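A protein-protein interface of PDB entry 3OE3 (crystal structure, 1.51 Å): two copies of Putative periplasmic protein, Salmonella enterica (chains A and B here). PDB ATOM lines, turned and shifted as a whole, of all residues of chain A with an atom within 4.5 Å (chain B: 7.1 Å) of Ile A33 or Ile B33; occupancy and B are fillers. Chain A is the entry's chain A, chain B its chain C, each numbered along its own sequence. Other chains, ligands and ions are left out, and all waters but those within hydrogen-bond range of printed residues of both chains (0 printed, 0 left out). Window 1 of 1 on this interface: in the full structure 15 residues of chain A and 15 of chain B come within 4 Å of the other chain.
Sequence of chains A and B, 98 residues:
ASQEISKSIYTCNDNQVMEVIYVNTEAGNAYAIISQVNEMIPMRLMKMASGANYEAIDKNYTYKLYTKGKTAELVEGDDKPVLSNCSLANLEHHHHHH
The side-chain carboxylate (OE1) of Glu A19 lies within hydrogen-bond range of the backbone NH (N) of Met B40 (2.8 Å). N of Met A40 is in hydrogen-bond range of OE1 of Glu B19 (3.0 Å).
Of the 11 printed residues of chain A, 7 touch a printed residue of chain B. Printed residues of chain A that touch a printed residue of chain B: Ile A5, Glu A19, Ile A21, Ile A33, Ile A34, Met A40 and Pro A42. Hydrophobic or aromatic side chains of chain A that line the printed part of chain B: Ile A5, Ile A21, Ile A33, Met A40 and Pro A42. Among the printed residues, 17 pairs touch across the chains. Among the printed residues, no Asp or Glu carboxylate lies within 4 Å of a Lys or Arg side-chain nitrogen of the other chain.
Ile A5 touches Pro B42, but with the chains exchanged Pro A42 does not touch Ile B5 (4.03 Å). Ile A21 touches Ile B33, but with the chains exchanged Ile A33 does not touch Ile B21 (4.5 Å). Ile A21 touches Met B40, and with the chains exchanged Met A40 touches Ile B21. Ile A33 touches Met B40, and with the chains exchanged Met A40 touches Ile B33. 11 positions are printed for both chains. Of the 17 pairs that touch across the chains among the printed residues, 12 have their exchanged pair printed and touching as well.
Ile B33 touches Ile A5. CB of Pro B42 touches CD1 of Ile A5, at 3.8 Å. Glu A19 touches Glu B39 (OE1 to CA, 3.5 Å). Ile A21 touches Pro B42 (CD1 to CG, 3.8 Å). CD1 of Ile A33 touches CD1 of Ile B33 (3.7 Å). Ile A33 touches Met B40 (O to CE, 3.3 Å). Ile B21 touches Met A40 (CG1 to CB, 3.9 Å). CE of Met A40 touches O of Ile B33, 3.5 Å away. Met A40 touches Met B40. CD1 of Ile B21 touches CG of Pro A42, 3.8 Å away.
Ile A33 touches just these residues of chain B: Ile B33 and Met B40. Ile B33 touches four residues of chain A. Printed residues of chain B within 4 Å of Glu A19: Glu B39 and Met B40. Printed residues of chain B within 4 Å of Pro A42: Ile B21 (3.8 Å). Of the printed residues of chain A, Tyr B31 touches Ile A5 (3.6 Å). Of the printed residues of chain A, Met B40 touches Glu A19, Ile A21, Ile A33, Ile A34 and Met A40. Ile A41 touches none of the printed residues of chain B. The nearest printed residue of chain A that does not touch Ile B33 is Val A23 (5.2 Å).
N of Ile A33 lies within hydrogen-bond range of O of Ile A21, at 2.7 Å. The backbone NH (N) of Ile A41 is in hydrogen-bond range of the backbone carbonyl oxygen (O) of Ile A34 (2.9 Å). O of Ile B21 is in hydrogen-bond range of N of Ile B33 (2.8 Å). N of Tyr B31 sits at hydrogen-bond distance from O of Val B23 (2.9 Å). The backbone carbonyl oxygen of Ile B34 lies within hydrogen-bond range of the backbone NH of Ile B41 (2.8 Å).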
ATOM      1  N   ILE A   5      -5.775 -37.495  23.787  1.00  0.00           N
ATOM      2  CA  ILE A   5      -6.313 -36.426  22.955  1.00  0.00           C
ATOM      3  C   ILE A   5      -5.543 -36.325  21.642  1.00  0.00           C
ATOM      4  O   ILE A   5      -4.332 -36.546  21.599  1.00  0.00           O
ATOM      5  CB  ILE A   5      -6.277 -35.096  23.736  1.00  0.00           C
ATOM      6  CG1 ILE A   5      -7.053 -34.011  23.014  1.00  0.00           C
ATOM      7  CG2 ILE A   5      -4.847 -34.690  24.000  1.00  0.00           C
ATOM      8  CD1 ILE A   5      -7.351 -32.823  23.928  1.00  0.00           C
ATOM      9  N   GLU A  19     -11.606 -28.472  11.641  1.00  0.00           N
ATOM     10  CA  GLU A  19     -10.777 -29.188  12.610  1.00  0.00           C
ATOM     11  C   GLU A  19     -11.644 -29.933  13.606  1.00  0.00           C
ATOM     12  O   GLU A  19     -12.725 -29.474  13.962  1.00  0.00           O
ATOM     13  CB  GLU A  19      -9.901 -28.229  13.402  1.00  0.00           C
ATOM     14  CG  GLU A  19      -8.927 -27.413  12.593  1.00  0.00           C
ATOM     15  CD  GLU A  19      -8.016 -26.631  13.513  1.00  0.00           C
ATOM     16  OE1 GLU A  19      -8.470 -26.310  14.631  1.00  0.00           O
ATOM     17  OE2 GLU A  19      -6.861 -26.347  13.132  1.00  0.00           O
ATOM     18  N   VAL A  20     -11.164 -31.086  14.059  1.00  0.00           N
ATOM     19  CA  VAL A  20     -11.839 -31.797  15.146  1.00  0.00           C
ATOM     20  C   VAL A  20     -10.809 -32.274  16.164  1.00  0.00           C
ATOM     21  O   VAL A  20      -9.796 -32.867  15.786  1.00  0.00           O
ATOM     22  CB  VAL A  20     -12.636 -33.032  14.654  1.00  0.00           C
ATOM     23  CG1 VAL A  20     -13.413 -33.636  15.802  1.00  0.00           C
ATOM     24  CG2 VAL A  20     -13.608 -32.665  13.506  1.00  0.00           C
ATOM     25  N   ILE A  21     -11.043 -31.992  17.448  1.00  0.00           N
ATOM     26  CA  ILE A  21     -10.222 -32.597  18.480  1.00  0.00           C
ATOM     27  C   ILE A  21     -10.964 -33.808  19.000  1.00  0.00           C
ATOM     28  O   ILE A  21     -12.124 -33.706  19.408  1.00  0.00           O
ATOM     29  CB  ILE A  21      -9.962 -31.642  19.661  1.00  0.00           C
ATOM     30  CG1 ILE A  21      -9.391 -30.303  19.166  1.00  0.00           C
ATOM     31  CG2 ILE A  21      -9.058 -32.325  20.683  1.00  0.00           C
ATOM     32  CD1 ILE A  21      -8.109 -30.409  18.352  1.00  0.00           C
ATOM     33  N   VAL A  23     -11.142 -37.021  21.682  1.00  0.00           N
ATOM     34  CA  VAL A  23     -10.686 -37.473  22.977  1.00  0.00           C
ATOM     35  C   VAL A  23     -11.137 -38.915  23.111  1.00  0.00           C
ATOM     36  O   VAL A  23     -12.271 -39.246  22.788  1.00  0.00           O
ATOM     37  CB  VAL A  23     -11.300 -36.648  24.129  1.00  0.00           C
ATOM     38  CG1 VAL A  23     -10.894 -37.236  25.479  1.00  0.00           C
ATOM     39  CG2 VAL A  23     -10.870 -35.183  24.026  1.00  0.00           C
ATOM     40  N   ALA A  32     -15.652 -35.507  20.958  1.00  0.00           N
ATOM     41  CA  ALA A  32     -15.084 -34.726  19.879  1.00  0.00           C
ATOM     42  C   ALA A  32     -15.380 -33.276  20.196  1.00  0.00           C
ATOM     43  O   ALA A  32     -16.404 -32.974  20.823  1.00  0.00           O
ATOM     44  CB  ALA A  32     -15.694 -35.104  18.559  1.00  0.00           C
ATOM     45  N   ILE A  33     -14.475 -32.386  19.800  1.00  0.00           N
ATOM     46  CA  ILE A  33     -14.714 -30.953  19.962  1.00  0.00           C
ATOM     47  C   ILE A  33     -14.536 -30.254  18.624  1.00  0.00           C
ATOM     48  O   ILE A  33     -13.524 -30.430  17.947  1.00  0.00           O
ATOM     49  CB  ILE A  33     -13.763 -30.308  20.981  1.00  0.00           C
ATOM     50  CG1 ILE A  33     -13.805 -31.051  22.327  1.00  0.00           C
ATOM     51  CG2 ILE A  33     -14.144 -28.833  21.162  1.00  0.00           C
ATOM     52  CD1 ILE A  33     -12.951 -32.313  22.389  1.00  0.00           C
ATOM     53  N   ILE A  34     -15.544 -29.474  18.232  1.00  0.00           N
ATOM     54  CA  ILE A  34     -15.452 -28.686  17.012  1.00  0.00           C
ATOM     55  C   ILE A  34     -15.482 -27.217  17.361  1.00  0.00           C
ATOM     56  O   ILE A  34     -15.720 -26.863  18.509  1.00  0.00           O
ATOM     57  CB  ILE A  34     -16.612 -28.994  16.055  1.00  0.00           C
ATOM     58  CG1 ILE A  34     -17.957 -28.765  16.744  1.00  0.00           C
ATOM     59  CG2 ILE A  34     -16.511 -30.438  15.549  1.00  0.00           C
ATOM     60  CD1 ILE A  34     -19.142 -28.895  15.797  1.00  0.00           C
ATOM     61  N   MET A  40     -16.148 -23.183  20.907  1.00  0.00           N
ATOM     62  CA  MET A  40     -15.814 -24.605  20.914  1.00  0.00           C
ATOM     63  C   MET A  40     -17.002 -25.364  21.494  1.00  0.00           C
ATOM     64  O   MET A  40     -17.581 -24.948  22.497  1.00  0.00           O
ATOM     65  CB  MET A  40     -14.526 -24.865  21.703  1.00  0.00           C
ATOM     66  CG  MET A  40     -13.265 -24.308  20.999  1.00  0.00           C
ATOM     67  SD  MET A  40     -11.636 -24.791  21.976  1.00  0.00           S
ATOM     68  CE  MET A  40     -11.746 -23.443  23.356  1.00  0.00           C
ATOM     69  N   ILE A  41     -17.378 -26.449  20.822  1.00  0.00           N
ATOM     70  CA  ILE A  41     -18.570 -27.221  21.142  1.00  0.00           C
ATOM     71  C   ILE A  41     -18.144 -28.660  21.452  1.00  0.00           C
ATOM     72  O   ILE A  41     -17.752 -29.393  20.547  1.00  0.00           O
ATOM     73  CB  ILE A  41     -19.511 -27.263  19.914  1.00  0.00           C
ATOM     74  CG1 ILE A  41     -19.786 -25.849  19.385  1.00  0.00           C
ATOM     75  CG2 ILE A  41     -20.830 -27.983  20.242  1.00  0.00           C
ATOM     76  CD1 ILE A  41     -20.517 -24.977  20.350  1.00  0.00           C
ATOM     77  N   PRO A  42     -18.192 -29.046  22.731  1.00  0.00           N
ATOM     78  CA  PRO A  42     -17.872 -30.436  23.068  1.00  0.00           C
ATOM     79  C   PRO A  42     -19.005 -31.356  22.658  1.00  0.00           C
ATOM     80  O   PRO A  42     -20.185 -30.986  22.788  1.00  0.00           O
ATOM     81  CB  PRO A  42     -17.749 -30.411  24.597  1.00  0.00           C
ATOM     82  CG  PRO A  42     -17.510 -28.975  24.959  1.00  0.00           C
ATOM     83  CD  PRO A  42     -18.221 -28.169  23.916  1.00  0.00           C
ATOM     84  N   ILE B   5     -15.768 -33.445  30.668  1.00  0.00           N
ATOM     85  CA  ILE B   5     -15.449 -32.308  29.818  1.00  0.00           C
ATOM     86  C   ILE B   5     -16.282 -31.105  30.254  1.00  0.00           C
ATOM     87  O   ILE B   5     -17.483 -31.223  30.524  1.00  0.00           O
ATOM     88  CB  ILE B   5     -15.673 -32.615  28.324  1.00  0.00           C
ATOM     89  CG1 ILE B   5     -14.958 -33.905  27.920  1.00  0.00           C
ATOM     90  CG2 ILE B   5     -15.130 -31.486  27.464  1.00  0.00           C
ATOM     91  CD1 ILE B   5     -14.545 -33.935  26.463  1.00  0.00           C
ATOM     92  N   GLU B  19     -11.945 -18.727  25.910  1.00  0.00           N
ATOM     93  CA  GLU B  19     -12.615 -19.991  26.184  1.00  0.00           C
ATOM     94  C   GLU B  19     -11.561 -21.087  26.382  1.00  0.00           C
ATOM     95  O   GLU B  19     -10.599 -21.180  25.624  1.00  0.00           O
ATOM     96  CB  GLU B  19     -13.492 -20.421  24.999  1.00  0.00           C
ATOM     97  CG  GLU B  19     -14.882 -19.849  24.957  1.00  0.00           C
ATOM     98  CD  GLU B  19     -15.745 -20.539  23.915  1.00  0.00           C
ATOM     99  OE1 GLU B  19     -15.248 -21.470  23.238  1.00  0.00           O
ATOM    100  OE2 GLU B  19     -16.920 -20.149  23.777  1.00  0.00           O
ATOM    101  N   VAL B  20     -11.761 -21.926  27.388  1.00  0.00           N
ATOM    102  CA  VAL B  20     -10.946 -23.121  27.537  1.00  0.00           C
ATOM    103  C   VAL B  20     -11.873 -24.313  27.731  1.00  0.00           C
ATOM    104  O   VAL B  20     -12.815 -24.255  28.516  1.00  0.00           O
ATOM    105  CB  VAL B  20      -9.975 -23.020  28.733  1.00  0.00           C
ATOM    106  CG1 VAL B  20      -9.049 -24.248  28.760  1.00  0.00           C
ATOM    107  CG2 VAL B  20      -9.142 -21.727  28.669  1.00  0.00           C
ATOM    108  N   ILE B  21     -11.619 -25.379  26.982  1.00  0.00           N
ATOM    109  CA  ILE B  21     -12.265 -26.661  27.235  1.00  0.00           C
ATOM    110  C   ILE B  21     -11.311 -27.473  28.098  1.00  0.00           C
ATOM    111  O   ILE B  21     -10.165 -27.693  27.714  1.00  0.00           O
ATOM    112  CB  ILE B  21     -12.552 -27.446  25.937  1.00  0.00           C
ATOM    113  CG1 ILE B  21     -13.430 -26.647  24.979  1.00  0.00           C
ATOM    114  CG2 ILE B  21     -13.214 -28.766  26.267  1.00  0.00           C
ATOM    115  CD1 ILE B  21     -14.800 -26.333  25.494  1.00  0.00           C
ATOM    116  N   TYR B  22     -11.766 -27.879  29.280  1.00  0.00           N
ATOM    117  CA  TYR B  22     -10.947 -28.718  30.133  1.00  0.00           C
ATOM    118  C   TYR B  22     -11.456 -30.152  30.079  1.00  0.00           C
ATOM    119  O   TYR B  22     -12.663 -30.390  30.144  1.00  0.00           O
ATOM    120  CB  TYR B  22     -10.999 -28.220  31.579  1.00  0.00           C
ATOM    121  CG  TYR B  22     -10.247 -26.918  31.808  1.00  0.00           C
ATOM    122  CD1 TYR B  22      -8.862 -26.890  31.777  1.00  0.00           C
ATOM    123  CD2 TYR B  22     -10.922 -25.736  32.086  1.00  0.00           C
ATOM    124  CE1 TYR B  22      -8.161 -25.720  32.005  1.00  0.00           C
ATOM    125  CE2 TYR B  22     -10.221 -24.542  32.325  1.00  0.00           C
ATOM    126  CZ  TYR B  22      -8.835 -24.551  32.272  1.00  0.00           C
ATOM    127  OH  TYR B  22      -8.096 -23.394  32.509  1.00  0.00           O
ATOM    128  N   VAL B  23     -10.524 -31.088  29.958  1.00  0.00           N
ATOM    129  CA  VAL B  23     -10.815 -32.518  29.990  1.00  0.00           C
ATOM    130  C   VAL B  23     -10.169 -33.082  31.245  1.00  0.00           C
ATOM    131  O   VAL B  23      -8.960 -32.977  31.440  1.00  0.00           O
ATOM    132  CB  VAL B  23     -10.245 -33.237  28.762  1.00  0.00           C
ATOM    133  CG1 VAL B  23     -10.557 -34.757  28.824  1.00  0.00           C
ATOM    134  CG2 VAL B  23     -10.802 -32.608  27.481  1.00  0.00           C
ATOM    135  N   TYR B  31      -6.288 -32.455  30.502  1.00  0.00           N
ATOM    136  CA  TYR B  31      -5.929 -31.812  29.244  1.00  0.00           C
ATOM    137  C   TYR B  31      -6.697 -30.506  29.157  1.00  0.00           C
ATOM    138  O   TYR B  31      -7.650 -30.278  29.915  1.00  0.00           O
ATOM    139  CB  TYR B  31      -6.288 -32.689  28.038  1.00  0.00           C
ATOM    140  CG  TYR B  31      -5.772 -34.107  28.134  1.00  0.00           C
ATOM    141  CD1 TYR B  31      -6.531 -35.095  28.750  1.00  0.00           C
ATOM    142  CD2 TYR B  31      -4.553 -34.468  27.584  1.00  0.00           C
ATOM    143  CE1 TYR B  31      -6.070 -36.394  28.843  1.00  0.00           C
ATOM    144  CE2 TYR B  31      -4.088 -35.778  27.664  1.00  0.00           C
ATOM    145  CZ  TYR B  31      -4.853 -36.731  28.299  1.00  0.00           C
ATOM    146  OH  TYR B  31      -4.430 -38.049  28.398  1.00  0.00           O
ATOM    147  N   ALA B  32      -6.287 -29.650  28.227  1.00  0.00           N
ATOM    148  CA  ALA B  32      -7.009 -28.414  27.958  1.00  0.00           C
ATOM    149  C   ALA B  32      -7.017 -28.180  26.467  1.00  0.00           C
ATOM    150  O   ALA B  32      -6.134 -28.642  25.758  1.00  0.00           O
ATOM    151  CB  ALA B  32      -6.339 -27.241  28.673  1.00  0.00           C
ATOM    152  N   ILE B  33      -8.024 -27.462  25.977  1.00  0.00           N
ATOM    153  CA  ILE B  33      -8.022 -27.051  24.583  1.00  0.00           C
ATOM    154  C   ILE B  33      -8.345 -25.573  24.522  1.00  0.00           C
ATOM    155  O   ILE B  33      -9.301 -25.114  25.140  1.00  0.00           O
ATOM    156  CB  ILE B  33      -9.069 -27.790  23.729  1.00  0.00           C
ATOM    157  CG1 ILE B  33      -8.962 -29.308  23.901  1.00  0.00           C
ATOM    158  CG2 ILE B  33      -8.884 -27.430  22.249  1.00  0.00           C
ATOM    159  CD1 ILE B  33     -10.203 -30.022  23.417  1.00  0.00           C
ATOM    160  N   ILE B  34      -7.524 -24.837  23.784  1.00  0.00           N
ATOM    161  CA  ILE B  34      -7.765 -23.410  23.539  1.00  0.00           C
ATOM    162  C   ILE B  34      -7.871 -23.164  22.042  1.00  0.00           C
ATOM    163  O   ILE B  34      -7.511 -24.020  21.247  1.00  0.00           O
ATOM    164  CB  ILE B  34      -6.644 -22.527  24.147  1.00  0.00           C
ATOM    165  CG1 ILE B  34      -5.296 -22.838  23.499  1.00  0.00           C
ATOM    166  CG2 ILE B  34      -6.605 -22.688  25.668  1.00  0.00           C
ATOM    167  CD1 ILE B  34      -4.165 -21.823  23.876  1.00  0.00           C
ATOM    168  N   SER B  35      -8.392 -22.002  21.656  1.00  0.00           N
ATOM    169  CA  SER B  35      -8.483 -21.633  20.257  1.00  0.00           C
ATOM    170  C   SER B  35      -7.673 -20.354  20.057  1.00  0.00           C
ATOM    171  O   SER B  35      -7.932 -19.348  20.713  1.00  0.00           O
ATOM    172  CB  SER B  35      -9.952 -21.414  19.880  1.00  0.00           C
ATOM    173  OG  SER B  35     -10.098 -21.025  18.531  1.00  0.00           O
ATOM    174  N   GLU B  39      -7.403 -21.734  15.215  1.00  0.00           N
ATOM    175  CA  GLU B  39      -7.050 -23.141  15.340  1.00  0.00           C
ATOM    176  C   GLU B  39      -7.277 -23.598  16.774  1.00  0.00           C
ATOM    177  O   GLU B  39      -7.024 -22.863  17.726  1.00  0.00           O
ATOM    178  CB  GLU B  39      -5.567 -23.369  15.008  1.00  0.00           C
ATOM    179  CG  GLU B  39      -5.134 -22.858  13.653  1.00  0.00           C
ATOM    180  CD  GLU B  39      -3.711 -23.245  13.324  1.00  0.00           C
ATOM    181  OE1 GLU B  39      -2.835 -23.151  14.210  1.00  0.00           O
ATOM    182  OE2 GLU B  39      -3.468 -23.639  12.165  1.00  0.00           O
ATOM    183  N   MET B  40      -7.706 -24.837  16.928  1.00  0.00           N
ATOM    184  CA  MET B  40      -7.770 -25.444  18.242  1.00  0.00           C
ATOM    185  C   MET B  40      -6.435 -26.114  18.588  1.00  0.00           C
ATOM    186  O   MET B  40      -5.852 -26.831  17.765  1.00  0.00           O
ATOM    187  CB  MET B  40      -8.907 -26.453  18.282  1.00  0.00           C
ATOM    188  CG  MET B  40     -10.274 -25.797  18.354  1.00  0.00           C
ATOM    189  SD  MET B  40     -11.717 -27.114  18.576  1.00  0.00           S
ATOM    190  CE  MET B  40     -11.535 -27.993  16.855  1.00  0.00           C
ATOM    191  N   ILE B  41      -5.958 -25.837  19.802  1.00  0.00           N
ATOM    192  CA  ILE B  41      -4.670 -26.319  20.275  1.00  0.00           C
ATOM    193  C   ILE B  41      -4.849 -27.218  21.503  1.00  0.00           C
ATOM    194  O   ILE B  41      -5.170 -26.750  22.596  1.00  0.00           O
ATOM    195  CB  ILE B  41      -3.731 -25.134  20.622  1.00  0.00           C
ATOM    196  CG1 ILE B  41      -3.646 -24.159  19.442  1.00  0.00           C
ATOM    197  CG2 ILE B  41      -2.340 -25.645  21.016  1.00  0.00           C
ATOM    198  CD1 ILE B  41      -2.953 -24.722  18.247  1.00  0.00           C
ATOM    199  N   PRO B  42      -4.694 -28.533  21.307  1.00  0.00           N
ATOM    200  CA  PRO B  42      -4.771 -29.441  22.460  1.00  0.00           C
ATOM    201  C   PRO B  42      -3.524 -29.319  23.326  1.00  0.00           C
ATOM    202  O   PRO B  42      -2.420 -29.187  22.796  1.00  0.00           O
ATOM    203  CB  PRO B  42      -4.825 -30.834  21.825  1.00  0.00           C
ATOM    204  CG  PRO B  42      -4.876 -30.652  20.359  1.00  0.00           C
ATOM    205  CD  PRO B  42      -4.565 -29.239  20.021  1.00  0.00           C
ATOM    206  N   MET B  43      -3.722 -29.348  24.641  1.00  0.00           N
ATOM    207  CA  MET B  43      -2.649 -29.175  25.607  1.00  0.00           C
ATOM    208  C   MET B  43      -2.693 -30.250  26.680  1.00  0.00           C
ATOM    209  O   MET B  43      -3.760 -30.778  26.993  1.00  0.00           O
ATOM    210  CB  MET B  43      -2.756 -27.802  26.250  1.00  0.00           C
ATOM    211  CG  MET B  43      -3.033 -26.716  25.240  1.00  0.00           C
ATOM    212  SD  MET B  43      -3.222 -24.986  26.124  1.00  0.00           S
ATOM    213  CE  MET B  43      -1.362 -24.512  26.245  1.00  0.00           C
ATOM    214  N   TYR B  54      -0.462 -25.968  31.598  1.00  0.00           N
ATOM    215  CA  TYR B  54      -0.611 -26.820  30.417  1.00  0.00           C
ATOM    216  C   TYR B  54       0.318 -26.387  29.298  1.00  0.00           C
ATOM    217  O   TYR B  54       0.635 -25.205  29.162  1.00  0.00           O
ATOM    218  CB  TYR B  54      -2.065 -26.794  29.910  1.00  0.00           C
ATOM    219  CG  TYR B  54      -3.111 -27.234  30.915  1.00  0.00           C
ATOM    220  CD1 TYR B  54      -3.553 -26.363  31.917  1.00  0.00           C
ATOM    221  CD2 TYR B  54      -3.662 -28.522  30.872  1.00  0.00           C
ATOM    222  CE1 TYR B  54      -4.504 -26.758  32.844  1.00  0.00           C
ATOM    223  CE2 TYR B  54      -4.620 -28.915  31.801  1.00  0.00           C
ATOM    224  CZ  TYR B  54      -5.035 -28.031  32.777  1.00  0.00           C
ATOM    225  OH  TYR B  54      -5.991 -28.414  33.693  1.00  0.00           O
ATOM    226  N   LEU B  65      -0.410 -22.460  29.081  1.00  0.00           N
ATOM    227  CA  LEU B  65      -1.513 -21.897  29.828  1.00  0.00           C
ATOM    228  C   LEU B  65      -1.216 -22.141  31.296  1.00  0.00           C
ATOM    229  O   LEU B  65      -1.100 -23.295  31.749  1.00  0.00           O
ATOM    230  CB  LEU B  65      -2.827 -22.593  29.408  1.00  0.00           C
ATOM    231  CG  LEU B  65      -4.078 -22.260  30.225  1.00  0.00           C
ATOM    232  CD1 LEU B  65      -4.478 -20.801  29.984  1.00  0.00           C
ATOM    233  CD2 LEU B  65      -5.245 -23.220  29.880  1.00  0.00           C
